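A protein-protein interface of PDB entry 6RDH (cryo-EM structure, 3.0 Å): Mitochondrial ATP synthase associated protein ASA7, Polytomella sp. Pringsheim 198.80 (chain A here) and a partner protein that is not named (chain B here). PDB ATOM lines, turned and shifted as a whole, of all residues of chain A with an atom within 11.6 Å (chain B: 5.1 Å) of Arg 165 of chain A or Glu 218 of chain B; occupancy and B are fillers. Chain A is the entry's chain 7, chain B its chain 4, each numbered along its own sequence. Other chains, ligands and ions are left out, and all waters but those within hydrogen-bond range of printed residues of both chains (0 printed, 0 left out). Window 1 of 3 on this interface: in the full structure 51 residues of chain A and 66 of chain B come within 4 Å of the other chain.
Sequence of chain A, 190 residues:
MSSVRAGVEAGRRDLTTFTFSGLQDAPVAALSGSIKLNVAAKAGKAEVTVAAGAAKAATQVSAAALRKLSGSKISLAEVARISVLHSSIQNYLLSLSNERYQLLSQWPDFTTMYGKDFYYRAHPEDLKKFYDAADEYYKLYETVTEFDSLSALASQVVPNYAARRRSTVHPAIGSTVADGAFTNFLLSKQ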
ATOM      1  N   LEU A  85      19.200  -7.157 -25.743  1.00  0.00           N
ATOM      2  CA  LEU A  85      19.802  -7.370 -24.434  1.00  0.00           C
ATOM      3  C   LEU A  85      21.205  -7.931 -24.565  1.00  0.00           C
ATOM      4  O   LEU A  85      22.141  -7.445 -23.915  1.00  0.00           O
ATOM      5  CB  LEU A  85      18.929  -8.319 -23.627  1.00  0.00           C
ATOM      6  CG  LEU A  85      19.554  -8.940 -22.401  1.00  0.00           C
ATOM      7  CD1 LEU A  85      19.748  -7.865 -21.408  1.00  0.00           C
ATOM      8  CD2 LEU A  85      18.677 -10.010 -21.839  1.00  0.00           C
ATOM      9  N   SER A  88      23.558  -5.296 -25.799  1.00  0.00           N
ATOM     10  CA  SER A  88      23.958  -4.358 -24.754  1.00  0.00           C
ATOM     11  C   SER A  88      25.033  -4.952 -23.860  1.00  0.00           C
ATOM     12  O   SER A  88      25.998  -4.268 -23.494  1.00  0.00           O
ATOM     13  CB  SER A  88      22.751  -3.963 -23.924  1.00  0.00           C
ATOM     14  OG  SER A  88      22.169  -5.118 -23.368  1.00  0.00           O
ATOM     15  N   ILE A  89      24.898  -6.235 -23.525  1.00  0.00           N
ATOM     16  CA  ILE A  89      25.912  -6.892 -22.703  1.00  0.00           C
ATOM     17  C   ILE A  89      27.218  -7.047 -23.475  1.00  0.00           C
ATOM     18  O   ILE A  89      28.306  -6.856 -22.922  1.00  0.00           O
ATOM     19  CB  ILE A  89      25.382  -8.237 -22.187  1.00  0.00           C
ATOM     20  CG1 ILE A  89      24.129  -8.003 -21.362  1.00  0.00           C
ATOM     21  CG2 ILE A  89      26.395  -8.921 -21.331  1.00  0.00           C
ATOM     22  CD1 ILE A  89      23.433  -9.241 -20.970  1.00  0.00           C
ATOM     23  N   TYR A  92      28.994  -3.797 -23.540  1.00  0.00           N
ATOM     24  CA  TYR A  92      29.702  -3.547 -22.290  1.00  0.00           C
ATOM     25  C   TYR A  92      30.981  -4.360 -22.201  1.00  0.00           C
ATOM     26  O   TYR A  92      31.999  -3.863 -21.715  1.00  0.00           O
ATOM     27  CB  TYR A  92      28.827  -3.856 -21.093  1.00  0.00           C
ATOM     28  CG  TYR A  92      29.468  -3.424 -19.813  1.00  0.00           C
ATOM     29  CD1 TYR A  92      29.835  -2.106 -19.626  1.00  0.00           C
ATOM     30  CD2 TYR A  92      29.716  -4.324 -18.801  1.00  0.00           C
ATOM     31  CE1 TYR A  92      30.422  -1.698 -18.469  1.00  0.00           C
ATOM     32  CE2 TYR A  92      30.300  -3.924 -17.634  1.00  0.00           C
ATOM     33  CZ  TYR A  92      30.654  -2.613 -17.475  1.00  0.00           C
ATOM     34  OH  TYR A  92      31.246  -2.201 -16.312  1.00  0.00           O
ATOM     35  N   VAL A 157      25.820 -14.138 -19.245  1.00  0.00           N
ATOM     36  CA  VAL A 157      25.227 -13.153 -18.351  1.00  0.00           C
ATOM     37  C   VAL A 157      23.735 -13.102 -18.640  1.00  0.00           C
ATOM     38  O   VAL A 157      22.934 -12.718 -17.786  1.00  0.00           O
ATOM     39  CB  VAL A 157      25.886 -11.780 -18.552  1.00  0.00           C
ATOM     40  CG1 VAL A 157      25.557 -10.858 -17.424  1.00  0.00           C
ATOM     41  CG2 VAL A 157      27.369 -11.931 -18.676  1.00  0.00           C
ATOM     42  N   VAL A 158      23.364 -13.508 -19.852  1.00  0.00           N
ATOM     43  CA  VAL A 158      21.959 -13.451 -20.267  1.00  0.00           C
ATOM     44  C   VAL A 158      21.038 -14.375 -19.478  1.00  0.00           C
ATOM     45  O   VAL A 158      19.977 -13.902 -19.027  1.00  0.00           O
ATOM     46  CB  VAL A 158      21.858 -13.658 -21.791  1.00  0.00           C
ATOM     47  CG1 VAL A 158      20.449 -13.951 -22.215  1.00  0.00           C
ATOM     48  CG2 VAL A 158      22.362 -12.451 -22.513  1.00  0.00           C
ATOM     49  N   PRO A 159      21.333 -15.679 -19.267  1.00  0.00           N
ATOM     50  CA  PRO A 159      20.300 -16.539 -18.663  1.00  0.00           C
ATOM     51  C   PRO A 159      19.978 -16.257 -17.205  1.00  0.00           C
ATOM     52  O   PRO A 159      18.802 -16.325 -16.836  1.00  0.00           O
ATOM     53  CB  PRO A 159      20.873 -17.948 -18.840  1.00  0.00           C
ATOM     54  CG  PRO A 159      21.793 -17.835 -19.920  1.00  0.00           C
ATOM     55  CD  PRO A 159      22.450 -16.544 -19.703  1.00  0.00           C
ATOM     56  N   ASN A 160      20.961 -15.920 -16.370  1.00  0.00           N
ATOM     57  CA  ASN A 160      20.662 -15.655 -14.965  1.00  0.00           C
ATOM     58  C   ASN A 160      19.907 -14.344 -14.793  1.00  0.00           C
ATOM     59  O   ASN A 160      18.986 -14.255 -13.971  1.00  0.00           O
ATOM     60  CB  ASN A 160      21.949 -15.635 -14.149  1.00  0.00           C
ATOM     61  CG  ASN A 160      22.471 -17.022 -13.861  1.00  0.00           C
ATOM     62  OD1 ASN A 160      21.757 -18.009 -14.013  1.00  0.00           O
ATOM     63  ND2 ASN A 160      23.716 -17.104 -13.419  1.00  0.00           N
ATOM     64  N   TYR A 161      20.278 -13.327 -15.571  1.00  0.00           N
ATOM     65  CA  TYR A 161      19.540 -12.072 -15.572  1.00  0.00           C
ATOM     66  C   TYR A 161      18.124 -12.271 -16.079  1.00  0.00           C
ATOM     67  O   TYR A 161      17.175 -11.730 -15.510  1.00  0.00           O
ATOM     68  CB  TYR A 161      20.261 -11.039 -16.434  1.00  0.00           C
ATOM     69  CG  TYR A 161      19.406  -9.852 -16.785  1.00  0.00           C
ATOM     70  CD1 TYR A 161      18.876  -9.701 -18.052  1.00  0.00           C
ATOM     71  CD2 TYR A 161      19.136  -8.875 -15.847  1.00  0.00           C
ATOM     72  CE1 TYR A 161      18.090  -8.632 -18.361  1.00  0.00           C
ATOM     73  CE2 TYR A 161      18.358  -7.798 -16.157  1.00  0.00           C
ATOM     74  CZ  TYR A 161      17.842  -7.682 -17.419  1.00  0.00           C
ATOM     75  OH  TYR A 161      17.062  -6.609 -17.757  1.00  0.00           O
ATOM     76  N   ALA A 162      17.963 -13.046 -17.145  1.00  0.00           N
ATOM     77  CA  ALA A 162      16.644 -13.241 -17.722  1.00  0.00           C
ATOM     78  C   ALA A 162      15.776 -14.130 -16.852  1.00  0.00           C
ATOM     79  O   ALA A 162      14.551 -14.096 -16.973  1.00  0.00           O
ATOM     80  CB  ALA A 162      16.765 -13.828 -19.122  1.00  0.00           C
ATOM     81  N   ALA A 163      16.382 -14.944 -15.993  1.00  0.00           N
ATOM     82  CA  ALA A 163      15.612 -15.673 -15.000  1.00  0.00           C
ATOM     83  C   ALA A 163      15.264 -14.817 -13.798  1.00  0.00           C
ATOM     84  O   ALA A 163      14.285 -15.110 -13.111  1.00  0.00           O
ATOM     85  CB  ALA A 163      16.373 -16.906 -14.538  1.00  0.00           C
ATOM     86  N   ARG A 164      16.046 -13.779 -13.518  1.00  0.00           N
ATOM     87  CA  ARG A 164      15.646 -12.849 -12.469  1.00  0.00           C
ATOM     88  C   ARG A 164      14.494 -11.960 -12.896  1.00  0.00           C
ATOM     89  O   ARG A 164      13.808 -11.411 -12.032  1.00  0.00           O
ATOM     90  CB  ARG A 164      16.826 -11.985 -12.049  1.00  0.00           C
ATOM     91  CG  ARG A 164      17.741 -12.671 -11.074  1.00  0.00           C
ATOM     92  CD  ARG A 164      18.827 -11.749 -10.593  1.00  0.00           C
ATOM     93  NE  ARG A 164      18.282 -10.524 -10.028  1.00  0.00           N
ATOM     94  CZ  ARG A 164      17.913 -10.397  -8.760  1.00  0.00           C
ATOM     95  NH1 ARG A 164      17.431  -9.247  -8.326  1.00  0.00           N
ATOM     96  NH2 ARG A 164      18.022 -11.421  -7.930  1.00  0.00           N
ATOM     97  N   ARG A 165      14.269 -11.796 -14.196  1.00  0.00           N
ATOM     98  CA  ARG A 165      13.176 -10.974 -14.688  1.00  0.00           C
ATOM     99  C   ARG A 165      11.926 -11.775 -14.985  1.00  0.00           C
ATOM    100  O   ARG A 165      10.916 -11.192 -15.382  1.00  0.00           O
ATOM    101  CB  ARG A 165      13.598 -10.211 -15.937  1.00  0.00           C
ATOM    102  CG  ARG A 165      14.777  -9.303 -15.736  1.00  0.00           C
ATOM    103  CD  ARG A 165      14.424  -8.035 -15.018  1.00  0.00           C
ATOM    104  NE  ARG A 165      14.584  -8.175 -13.583  1.00  0.00           N
ATOM    105  CZ  ARG A 165      14.761  -7.166 -12.746  1.00  0.00           C
ATOM    106  NH1 ARG A 165      14.889  -7.402 -11.449  1.00  0.00           N
ATOM    107  NH2 ARG A 165      14.825  -5.925 -13.198  1.00  0.00           N
ATOM    108  N   ARG A 166      11.971 -13.090 -14.821  1.00  0.00           N
ATOM    109  CA  ARG A 166      10.763 -13.904 -14.801  1.00  0.00           C
ATOM    110  C   ARG A 166      10.293 -14.066 -13.364  1.00  0.00           C
ATOM    111  O   ARG A 166      10.178 -15.159 -12.836  1.00  0.00           O
ATOM    112  CB  ARG A 166      11.013 -15.257 -15.445  1.00  0.00           C
ATOM    113  CG  ARG A 166      10.919 -15.260 -16.936  1.00  0.00           C
ATOM    114  CD  ARG A 166      10.927 -16.675 -17.437  1.00  0.00           C
ATOM    115  NE  ARG A 166      12.036 -17.422 -16.867  1.00  0.00           N
ATOM    116  CZ  ARG A 166      13.235 -17.507 -17.423  1.00  0.00           C
ATOM    117  NH1 ARG A 166      14.190 -18.208 -16.837  1.00  0.00           N
ATOM    118  NH2 ARG A 166      13.479 -16.890 -18.564  1.00  0.00           N
ATOM    119  N   SER A 167      10.042 -12.938 -12.728  1.00  0.00           N
ATOM    120  CA  SER A 167       9.617 -12.954 -11.346  1.00  0.00           C
ATOM    121  C   SER A 167       8.118 -13.164 -11.283  1.00  0.00           C
ATOM    122  O   SER A 167       7.376 -12.757 -12.176  1.00  0.00           O
ATOM    123  CB  SER A 167      10.003 -11.660 -10.642  1.00  0.00           C
ATOM    124  OG  SER A 167       9.584 -11.675  -9.295  1.00  0.00           O
ATOM    125  N   THR A 168       7.679 -13.833 -10.229  1.00  0.00           N
ATOM    126  CA  THR A 168       6.264 -14.071 -10.023  1.00  0.00           C
ATOM    127  C   THR A 168       5.517 -12.817  -9.600  1.00  0.00           C
ATOM    128  O   THR A 168       4.287 -12.794  -9.681  1.00  0.00           O
ATOM    129  CB  THR A 168       6.076 -15.160  -8.978  1.00  0.00           C
ATOM    130  OG1 THR A 168       6.641 -14.725  -7.736  1.00  0.00           O
ATOM    131  CG2 THR A 168       6.777 -16.419  -9.413  1.00  0.00           C
ATOM    132  N   VAL A 169       6.224 -11.783  -9.155  1.00  0.00           N
ATOM    133  CA  VAL A 169       5.598 -10.525  -8.787  1.00  0.00           C
ATOM    134  C   VAL A 169       5.551  -9.601  -9.991  1.00  0.00           C
ATOM    135  O   VAL A 169       4.479  -9.320 -10.521  1.00  0.00           O
ATOM    136  CB  VAL A 169       6.351  -9.865  -7.627  1.00  0.00           C
ATOM    137  CG1 VAL A 169       5.706  -8.565  -7.264  1.00  0.00           C
ATOM    138  CG2 VAL A 169       6.381 -10.787  -6.449  1.00  0.00           C
ATOM    139  N   HIS A 170       6.711  -9.172 -10.473  1.00  0.00           N
ATOM    140  CA  HIS A 170       6.770  -8.195 -11.550  1.00  0.00           C
ATOM    141  C   HIS A 170       8.155  -8.257 -12.161  1.00  0.00           C
ATOM    142  O   HIS A 170       9.115  -8.580 -11.457  1.00  0.00           O
ATOM    143  CB  HIS A 170       6.474  -6.783 -11.029  1.00  0.00           C
ATOM    144  CG  HIS A 170       6.076  -5.811 -12.093  1.00  0.00           C
ATOM    145  ND1 HIS A 170       4.779  -5.667 -12.525  1.00  0.00           N
ATOM    146  CD2 HIS A 170       6.808  -4.934 -12.813  1.00  0.00           C
ATOM    147  CE1 HIS A 170       4.731  -4.743 -13.467  1.00  0.00           C
ATOM    148  NE2 HIS A 170       5.949  -4.282 -13.660  1.00  0.00           N
ATOM    149  N   PRO A 171       8.293  -7.982 -13.460  1.00  0.00           N
ATOM    150  CA  PRO A 171       9.636  -7.881 -14.047  1.00  0.00           C
ATOM    151  C   PRO A 171      10.462  -6.739 -13.500  1.00  0.00           C
ATOM    152  O   PRO A 171      11.692  -6.832 -13.491  1.00  0.00           O
ATOM    153  CB  PRO A 171       9.347  -7.678 -15.535  1.00  0.00           C
ATOM    154  CG  PRO A 171       8.021  -8.226 -15.740  1.00  0.00           C
ATOM    155  CD  PRO A 171       7.252  -8.038 -14.494  1.00  0.00           C
ATOM    156  N   ALA A 172       9.832  -5.663 -13.048  1.00  0.00           N
ATOM    157  CA  ALA A 172      10.527  -4.466 -12.611  1.00  0.00           C
ATOM    158  C   ALA A 172      10.584  -4.330 -11.102  1.00  0.00           C
ATOM    159  O   ALA A 172      10.959  -3.267 -10.606  1.00  0.00           O
ATOM    160  CB  ALA A 172       9.864  -3.224 -13.199  1.00  0.00           C
ATOM    161  N   ILE A 173      10.220  -5.359 -10.367  1.00  0.00           N
ATOM    162  CA  ILE A 173      10.171  -5.256  -8.917  1.00  0.00           C
ATOM    163  C   ILE A 173      11.586  -5.333  -8.366  1.00  0.00           C
ATOM    164  O   ILE A 173      12.488  -5.915  -8.975  1.00  0.00           O
ATOM    165  CB  ILE A 173       9.240  -6.339  -8.327  1.00  0.00           C
ATOM    166  CG1 ILE A 173       8.757  -5.957  -6.934  1.00  0.00           C
ATOM    167  CG2 ILE A 173       9.900  -7.705  -8.293  1.00  0.00           C
ATOM    168  CD1 ILE A 173       8.161  -4.596  -6.847  1.00  0.00           C
ATOM    169  N   GLY A 174      11.801  -4.678  -7.235  1.00  0.00           N
ATOM    170  CA  GLY A 174      13.095  -4.698  -6.600  1.00  0.00           C
ATOM    171  C   GLY A 174      12.945  -4.678  -5.102  1.00  0.00           C
ATOM    172  O   GLY A 174      11.843  -4.875  -4.594  1.00  0.00           O
ATOM    173  N   SER A 175      14.034  -4.436  -4.377  1.00  0.00           N
ATOM    174  CA  SER A 175      13.948  -4.448  -2.926  1.00  0.00           C
ATOM    175  C   SER A 175      13.417  -3.143  -2.361  1.00  0.00           C
ATOM    176  O   SER A 175      12.759  -3.162  -1.321  1.00  0.00           O
ATOM    177  CB  SER A 175      15.305  -4.765  -2.314  1.00  0.00           C
ATOM    178  OG  SER A 175      15.649  -6.112  -2.556  1.00  0.00           O
ATOM    179  N   THR A 176      13.665  -2.011  -3.016  1.00  0.00           N
ATOM    180  CA  THR A 176      13.208  -0.744  -2.456  1.00  0.00           C
ATOM    181  C   THR A 176      11.695  -0.605  -2.560  1.00  0.00           C
ATOM    182  O   THR A 176      11.042  -0.202  -1.593  1.00  0.00           O
ATOM    183  CB  THR A 176      13.896   0.422  -3.147  1.00  0.00           C
ATOM    184  OG1 THR A 176      15.310   0.209  -3.129  1.00  0.00           O
ATOM    185  CG2 THR A 176      13.617   1.699  -2.397  1.00  0.00           C
ATOM    186  N   VAL A 177      11.116  -0.960  -3.710  1.00  0.00           N
ATOM    187  CA  VAL A 177       9.668  -0.872  -3.872  1.00  0.00           C
ATOM    188  C   VAL A 177       8.971  -1.903  -3.002  1.00  0.00           C
ATOM    189  O   VAL A 177       7.923  -1.623  -2.417  1.00  0.00           O
ATOM    190  CB  VAL A 177       9.272  -1.031  -5.350  1.00  0.00           C
ATOM    191  CG1 VAL A 177       7.810  -0.744  -5.537  1.00  0.00           C
ATOM    192  CG2 VAL A 177      10.069  -0.115  -6.211  1.00  0.00           C
ATOM    193  N   ALA A 178       9.546  -3.095  -2.875  1.00  0.00           N
ATOM    194  CA  ALA A 178       8.922  -4.103  -2.030  1.00  0.00           C
ATOM    195  C   ALA A 178       9.025  -3.743  -0.555  1.00  0.00           C
ATOM    196  O   ALA A 178       8.093  -4.014   0.208  1.00  0.00           O
ATOM    197  CB  ALA A 178       9.539  -5.470  -2.290  1.00  0.00           C
ATOM    198  N   VAL B  63       6.571 -11.661 -21.078  1.00  0.00           N
ATOM    199  CA  VAL B  63       7.647 -11.030 -20.324  1.00  0.00           C
ATOM    200  C   VAL B  63       8.994 -11.386 -20.913  1.00  0.00           C
ATOM    201  O   VAL B  63       9.798 -10.501 -21.224  1.00  0.00           O
ATOM    202  CB  VAL B  63       7.570 -11.419 -18.836  1.00  0.00           C
ATOM    203  CG1 VAL B  63       8.894 -11.209 -18.140  1.00  0.00           C
ATOM    204  CG2 VAL B  63       6.567 -10.591 -18.154  1.00  0.00           C
ATOM    205  N   VAL B  67      11.889  -9.113 -22.448  1.00  0.00           N
ATOM    206  CA  VAL B  67      13.081  -8.727 -21.697  1.00  0.00           C
ATOM    207  C   VAL B  67      14.269  -8.617 -22.637  1.00  0.00           C
ATOM    208  O   VAL B  67      15.050  -7.664 -22.570  1.00  0.00           O
ATOM    209  CB  VAL B  67      13.339  -9.725 -20.553  1.00  0.00           C
ATOM    210  CG1 VAL B  67      14.774  -9.685 -20.089  1.00  0.00           C
ATOM    211  CG2 VAL B  67      12.444  -9.413 -19.392  1.00  0.00           C
ATOM    212  N   TYR B  85      15.391   2.175 -18.840  1.00  0.00           N
ATOM    213  CA  TYR B  85      15.375   0.740 -18.597  1.00  0.00           C
ATOM    214  C   TYR B  85      14.233   0.352 -17.678  1.00  0.00           C
ATOM    215  O   TYR B  85      13.496  -0.602 -17.955  1.00  0.00           O
ATOM    216  CB  TYR B  85      16.715   0.323 -18.011  1.00  0.00           C
ATOM    217  CG  TYR B  85      16.782  -1.075 -17.489  1.00  0.00           C
ATOM    218  CD1 TYR B  85      17.068  -1.316 -16.162  1.00  0.00           C
ATOM    219  CD2 TYR B  85      16.589  -2.154 -18.325  1.00  0.00           C
ATOM    220  CE1 TYR B  85      17.142  -2.585 -15.678  1.00  0.00           C
ATOM    221  CE2 TYR B  85      16.658  -3.428 -17.848  1.00  0.00           C
ATOM    222  CZ  TYR B  85      16.939  -3.635 -16.524  1.00  0.00           C
ATOM    223  OH  TYR B  85      17.015  -4.905 -16.030  1.00  0.00           O
ATOM    224  N   LEU B  89      10.821  -1.812 -18.534  1.00  0.00           N
ATOM    225  CA  LEU B  89      10.355  -2.941 -17.735  1.00  0.00           C
ATOM    226  C   LEU B  89       8.942  -2.715 -17.205  1.00  0.00           C
ATOM    227  O   LEU B  89       8.154  -3.663 -17.127  1.00  0.00           O
ATOM    228  CB  LEU B  89      11.322  -3.201 -16.591  1.00  0.00           C
ATOM    229  CG  LEU B  89      12.682  -3.800 -16.916  1.00  0.00           C
ATOM    230  CD1 LEU B  89      13.474  -3.938 -15.653  1.00  0.00           C
ATOM    231  CD2 LEU B  89      12.532  -5.137 -17.571  1.00  0.00           C
ATOM    232  N   ASP B 214      16.371   0.385  -7.793  1.00  0.00           N
ATOM    233  CA  ASP B 214      16.337  -1.057  -8.032  1.00  0.00           C
ATOM    234  C   ASP B 214      16.913  -1.420  -9.393  1.00  0.00           C
ATOM    235  O   ASP B 214      17.655  -2.406  -9.518  1.00  0.00           O
ATOM    236  CB  ASP B 214      14.911  -1.572  -7.928  1.00  0.00           C
ATOM    237  CG  ASP B 214      14.359  -1.445  -6.547  1.00  0.00           C
ATOM    238  OD1 ASP B 214      15.158  -1.447  -5.592  1.00  0.00           O
ATOM    239  OD2 ASP B 214      13.126  -1.356  -6.414  1.00  0.00           O
ATOM    240  N   ALA B 215      16.578  -0.645 -10.424  1.00  0.00           N
ATOM    241  CA  ALA B 215      17.127  -0.899 -11.748  1.00  0.00           C
ATOM    242  C   ALA B 215      18.622  -0.635 -11.783  1.00  0.00           C
ATOM    243  O   ALA B 215      19.363  -1.361 -12.446  1.00  0.00           O
ATOM    244  CB  ALA B 215      16.409  -0.047 -12.787  1.00  0.00           C
ATOM    245  N   ALA B 216      19.090   0.374 -11.049  1.00  0.00           N
ATOM    246  CA  ALA B 216      20.518   0.623 -10.971  1.00  0.00           C
ATOM    247  C   ALA B 216      21.238  -0.464 -10.191  1.00  0.00           C
ATOM    248  O   ALA B 216      22.389  -0.768 -10.499  1.00  0.00           O
ATOM    249  CB  ALA B 216      20.771   1.991 -10.349  1.00  0.00           C
ATOM    250  N   ALA B 217      20.587  -1.082  -9.206  1.00  0.00           N
ATOM    251  CA  ALA B 217      21.214  -2.213  -8.529  1.00  0.00           C
ATOM    252  C   ALA B 217      21.313  -3.426  -9.445  1.00  0.00           C
ATOM    253  O   ALA B 217      22.321  -4.142  -9.424  1.00  0.00           O
ATOM    254  CB  ALA B 217      20.448  -2.565  -7.263  1.00  0.00           C
ATOM    255  N   GLU B 218      20.286  -3.661 -10.271  1.00  0.00           N
ATOM    256  CA  GLU B 218      20.361  -4.734 -11.266  1.00  0.00           C
ATOM    257  C   GLU B 218      21.435  -4.478 -12.312  1.00  0.00           C
ATOM    258  O   GLU B 218      22.172  -5.401 -12.677  1.00  0.00           O
ATOM    259  CB  GLU B 218      19.015  -4.910 -11.963  1.00  0.00           C
ATOM    260  CG  GLU B 218      17.908  -5.411 -11.070  1.00  0.00           C
ATOM    261  CD  GLU B 218      18.020  -6.889 -10.760  1.00  0.00           C
ATOM    262  OE1 GLU B 218      18.468  -7.651 -11.640  1.00  0.00           O
ATOM    263  OE2 GLU B 218      17.655  -7.292  -9.638  1.00  0.00           O
ATOM    264  N   VAL B 219      21.553  -3.233 -12.777  1.00  0.00           N
ATOM    265  CA  VAL B 219      22.586  -2.866 -13.742  1.00  0.00           C
ATOM    266  C   VAL B 219      23.971  -2.989 -13.120  1.00  0.00           C
ATOM    267  O   VAL B 219      24.910  -3.455 -13.767  1.00  0.00           O
ATOM    268  CB  VAL B 219      22.319  -1.448 -14.278  1.00  0.00           C
ATOM    269  CG1 VAL B 219      23.513  -0.872 -14.992  1.00  0.00           C
ATOM    270  CG2 VAL B 219      21.147  -1.470 -15.197  1.00  0.00           C
ATOM    271  N   LYS B 220      24.111  -2.633 -11.844  1.00  0.00           N
ATOM    272  CA  LYS B 220      25.411  -2.736 -11.193  1.00  0.00           C
ATOM    273  C   LYS B 220      25.813  -4.183 -10.986  1.00  0.00           C
ATOM    274  O   LYS B 220      26.992  -4.523 -11.114  1.00  0.00           O
ATOM    275  CB  LYS B 220      25.408  -1.995  -9.859  1.00  0.00           C
ATOM    276  CG  LYS B 220      26.164  -0.687  -9.894  1.00  0.00           C
ATOM    277  CD  LYS B 220      25.583   0.239 -10.948  1.00  0.00           C
ATOM    278  CE  LYS B 220      26.566   1.306 -11.368  1.00  0.00           C
ATOM    279  NZ  LYS B 220      26.074   2.040 -12.566  1.00  0.00           N
ATOM    280  N   ALA B 221      24.852  -5.058 -10.704  1.00  0.00           N
ATOM    281  CA  ALA B 221      25.202  -6.467 -10.586  1.00  0.00           C
ATOM    282  C   ALA B 221      25.538  -7.086 -11.931  1.00  0.00           C
ATOM    283  O   ALA B 221      26.414  -7.950 -12.001  1.00  0.00           O
ATOM    284  CB  ALA B 221      24.078  -7.246  -9.937  1.00  0.00           C
ATOM    285  N   ILE B 222      24.876  -6.660 -13.006  1.00  0.00           N
ATOM    286  CA  ILE B 222      25.232  -7.196 -14.317  1.00  0.00           C
ATOM    287  C   ILE B 222      26.582  -6.651 -14.772  1.00  0.00           C
ATOM    288  O   ILE B 222      27.369  -7.372 -15.393  1.00  0.00           O
ATOM    289  CB  ILE B 222      24.103  -6.910 -15.322  1.00  0.00           C
ATOM    290  CG1 ILE B 222      22.856  -7.681 -14.918  1.00  0.00           C
ATOM    291  CG2 ILE B 222      24.469  -7.342 -16.713  1.00  0.00           C
ATOM    292  CD1 ILE B 222      23.075  -9.164 -14.790  1.00  0.00           C
ATOM    293  N   GLU B 223      26.896  -5.404 -14.421  1.00  0.00           N
ATOM    294  CA  GLU B 223      28.211  -4.838 -14.697  1.00  0.00           C
ATOM    295  C   GLU B 223      29.302  -5.592 -13.959  1.00  0.00           C
ATOM    296  O   GLU B 223      30.345  -5.918 -14.535  1.00  0.00           O
ATOM    297  CB  GLU B 223      28.247  -3.372 -14.288  1.00  0.00           C
ATOM    298  CG  GLU B 223      27.686  -2.425 -15.290  1.00  0.00           C
ATOM    299  CD  GLU B 223      27.752  -1.002 -14.816  1.00  0.00           C
ATOM    300  OE1 GLU B 223      28.046  -0.785 -13.628  1.00  0.00           O
ATOM    301  OE2 GLU B 223      27.508  -0.095 -15.627  1.00  0.00           O
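OD1 of Asp 214 of chain B lies within hydrogen-bond range of OG1 of Thr 176 of chain A, 3.0 Å away. OD2 of Asp 214 of chain B lies close to N of Val 177 of chain A (3.4 Å). OD1 of Asp 214 of chain B sits at hydrogen-bond distance from N of Ser 175 of chain A (3.4 Å). OE1 of Glu 218 of chain B is in salt-bridge range of NE of Arg 164 of chain A, 3.3 Å away. OH of Tyr 161 of chain A is in hydrogen-bond range of OH of Tyr 85 of chain B (2.4 Å). The side-chain carboxylate of Glu 218 of chain B lies within salt-bridge range of the guanidinium group of Arg 165 of chain A, 3.3 Å away.
NE of Arg 165 of chain A sits close to O of Pro 171 of chain A (3.2 Å). OE1 of Glu 223 of chain B is in salt-bridge range of NZ of Lys 220 of chain B.
Among the printed residues, merely in contact across the chains: Tyr 92 of chain A with Glu 223 of chain B, Val 157 of chain A with Ile 222 of chain B, Tyr 161 of chain A with Val 67 of chain B, Tyr 161 of chain A with Ile 222 of chain B, Arg 165 of chain A with Val 63 of chain B, Arg 165 of chain A with Val 67 of chain B, Arg 165 of chain A with Tyr 85 of chain B, Arg 165 of chain A with Leu 89 of chain B, Pro 171 of chain A with Val 63 of chain B, Ala 172 of chain A with Leu 89 of chain B and Gly 174 of chain A with Asp 214 of chain B.
Printed residues of chain B within 4 Å of Arg 164 of chain A: Glu 218 (2.4 Å). Arg 165 of chain A touches just these residues of chain B: Val 63, Val 67, Tyr 85, Leu 89 and Glu 218. Arg 166 of chain A touches none of the printed residues of chain B. Of the printed residues of chain B, Ala 172 of chain A touches Leu 89. Val 63 of chain B touches two residues of chain A. Val 67 of chain B touches just these residues of chain A: Tyr 161 and Arg 165. Of the printed residues of chain A, Tyr 85 of chain B touches Tyr 161 (2.4 Å) and Arg 165 (3.7 Å). No residue of chain A comes within 4 Å of Ala 217 of chain B. Of chain A, only Arg 164 (2.4 Å) and Arg 165 (3.2 Å) come within 4 Å of Glu 218 of chain B. No residue of chain A comes within 4 Å of Val 219 of chain B. No residue of chain A comes within 4 Å of Ala 221 of chain B. Ile 222 of chain B touches two residues of chain A. Printed residues of chain A within 4 Å of Glu 223 of chain B: Tyr 92.
Printed residues of chain A that touch a printed residue of chain B: Tyr 92, Val 157, Tyr 161, Arg 164, Arg 165, Pro 171, Ala 172, Gly 174, Ser 175, Thr 176 and Val 177. Of the 14 printed residues of chain B, 8 touch a printed residue of chain A. Hydrophobic or aromatic side chains of chain B within 4 Å of the printed part of chain A: Val 63, Val 67, Tyr 85, Leu 89 and Ile 222. Among the printed residues, Asp or Glu carboxylates within 4 Å of a Lys or Arg side-chain nitrogen of the other chain: Arg 164 of chain A with Glu 218 of chain B (2.4 Å) and Arg 165 of chain A with Glu 218 of chain B (3.3 Å).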
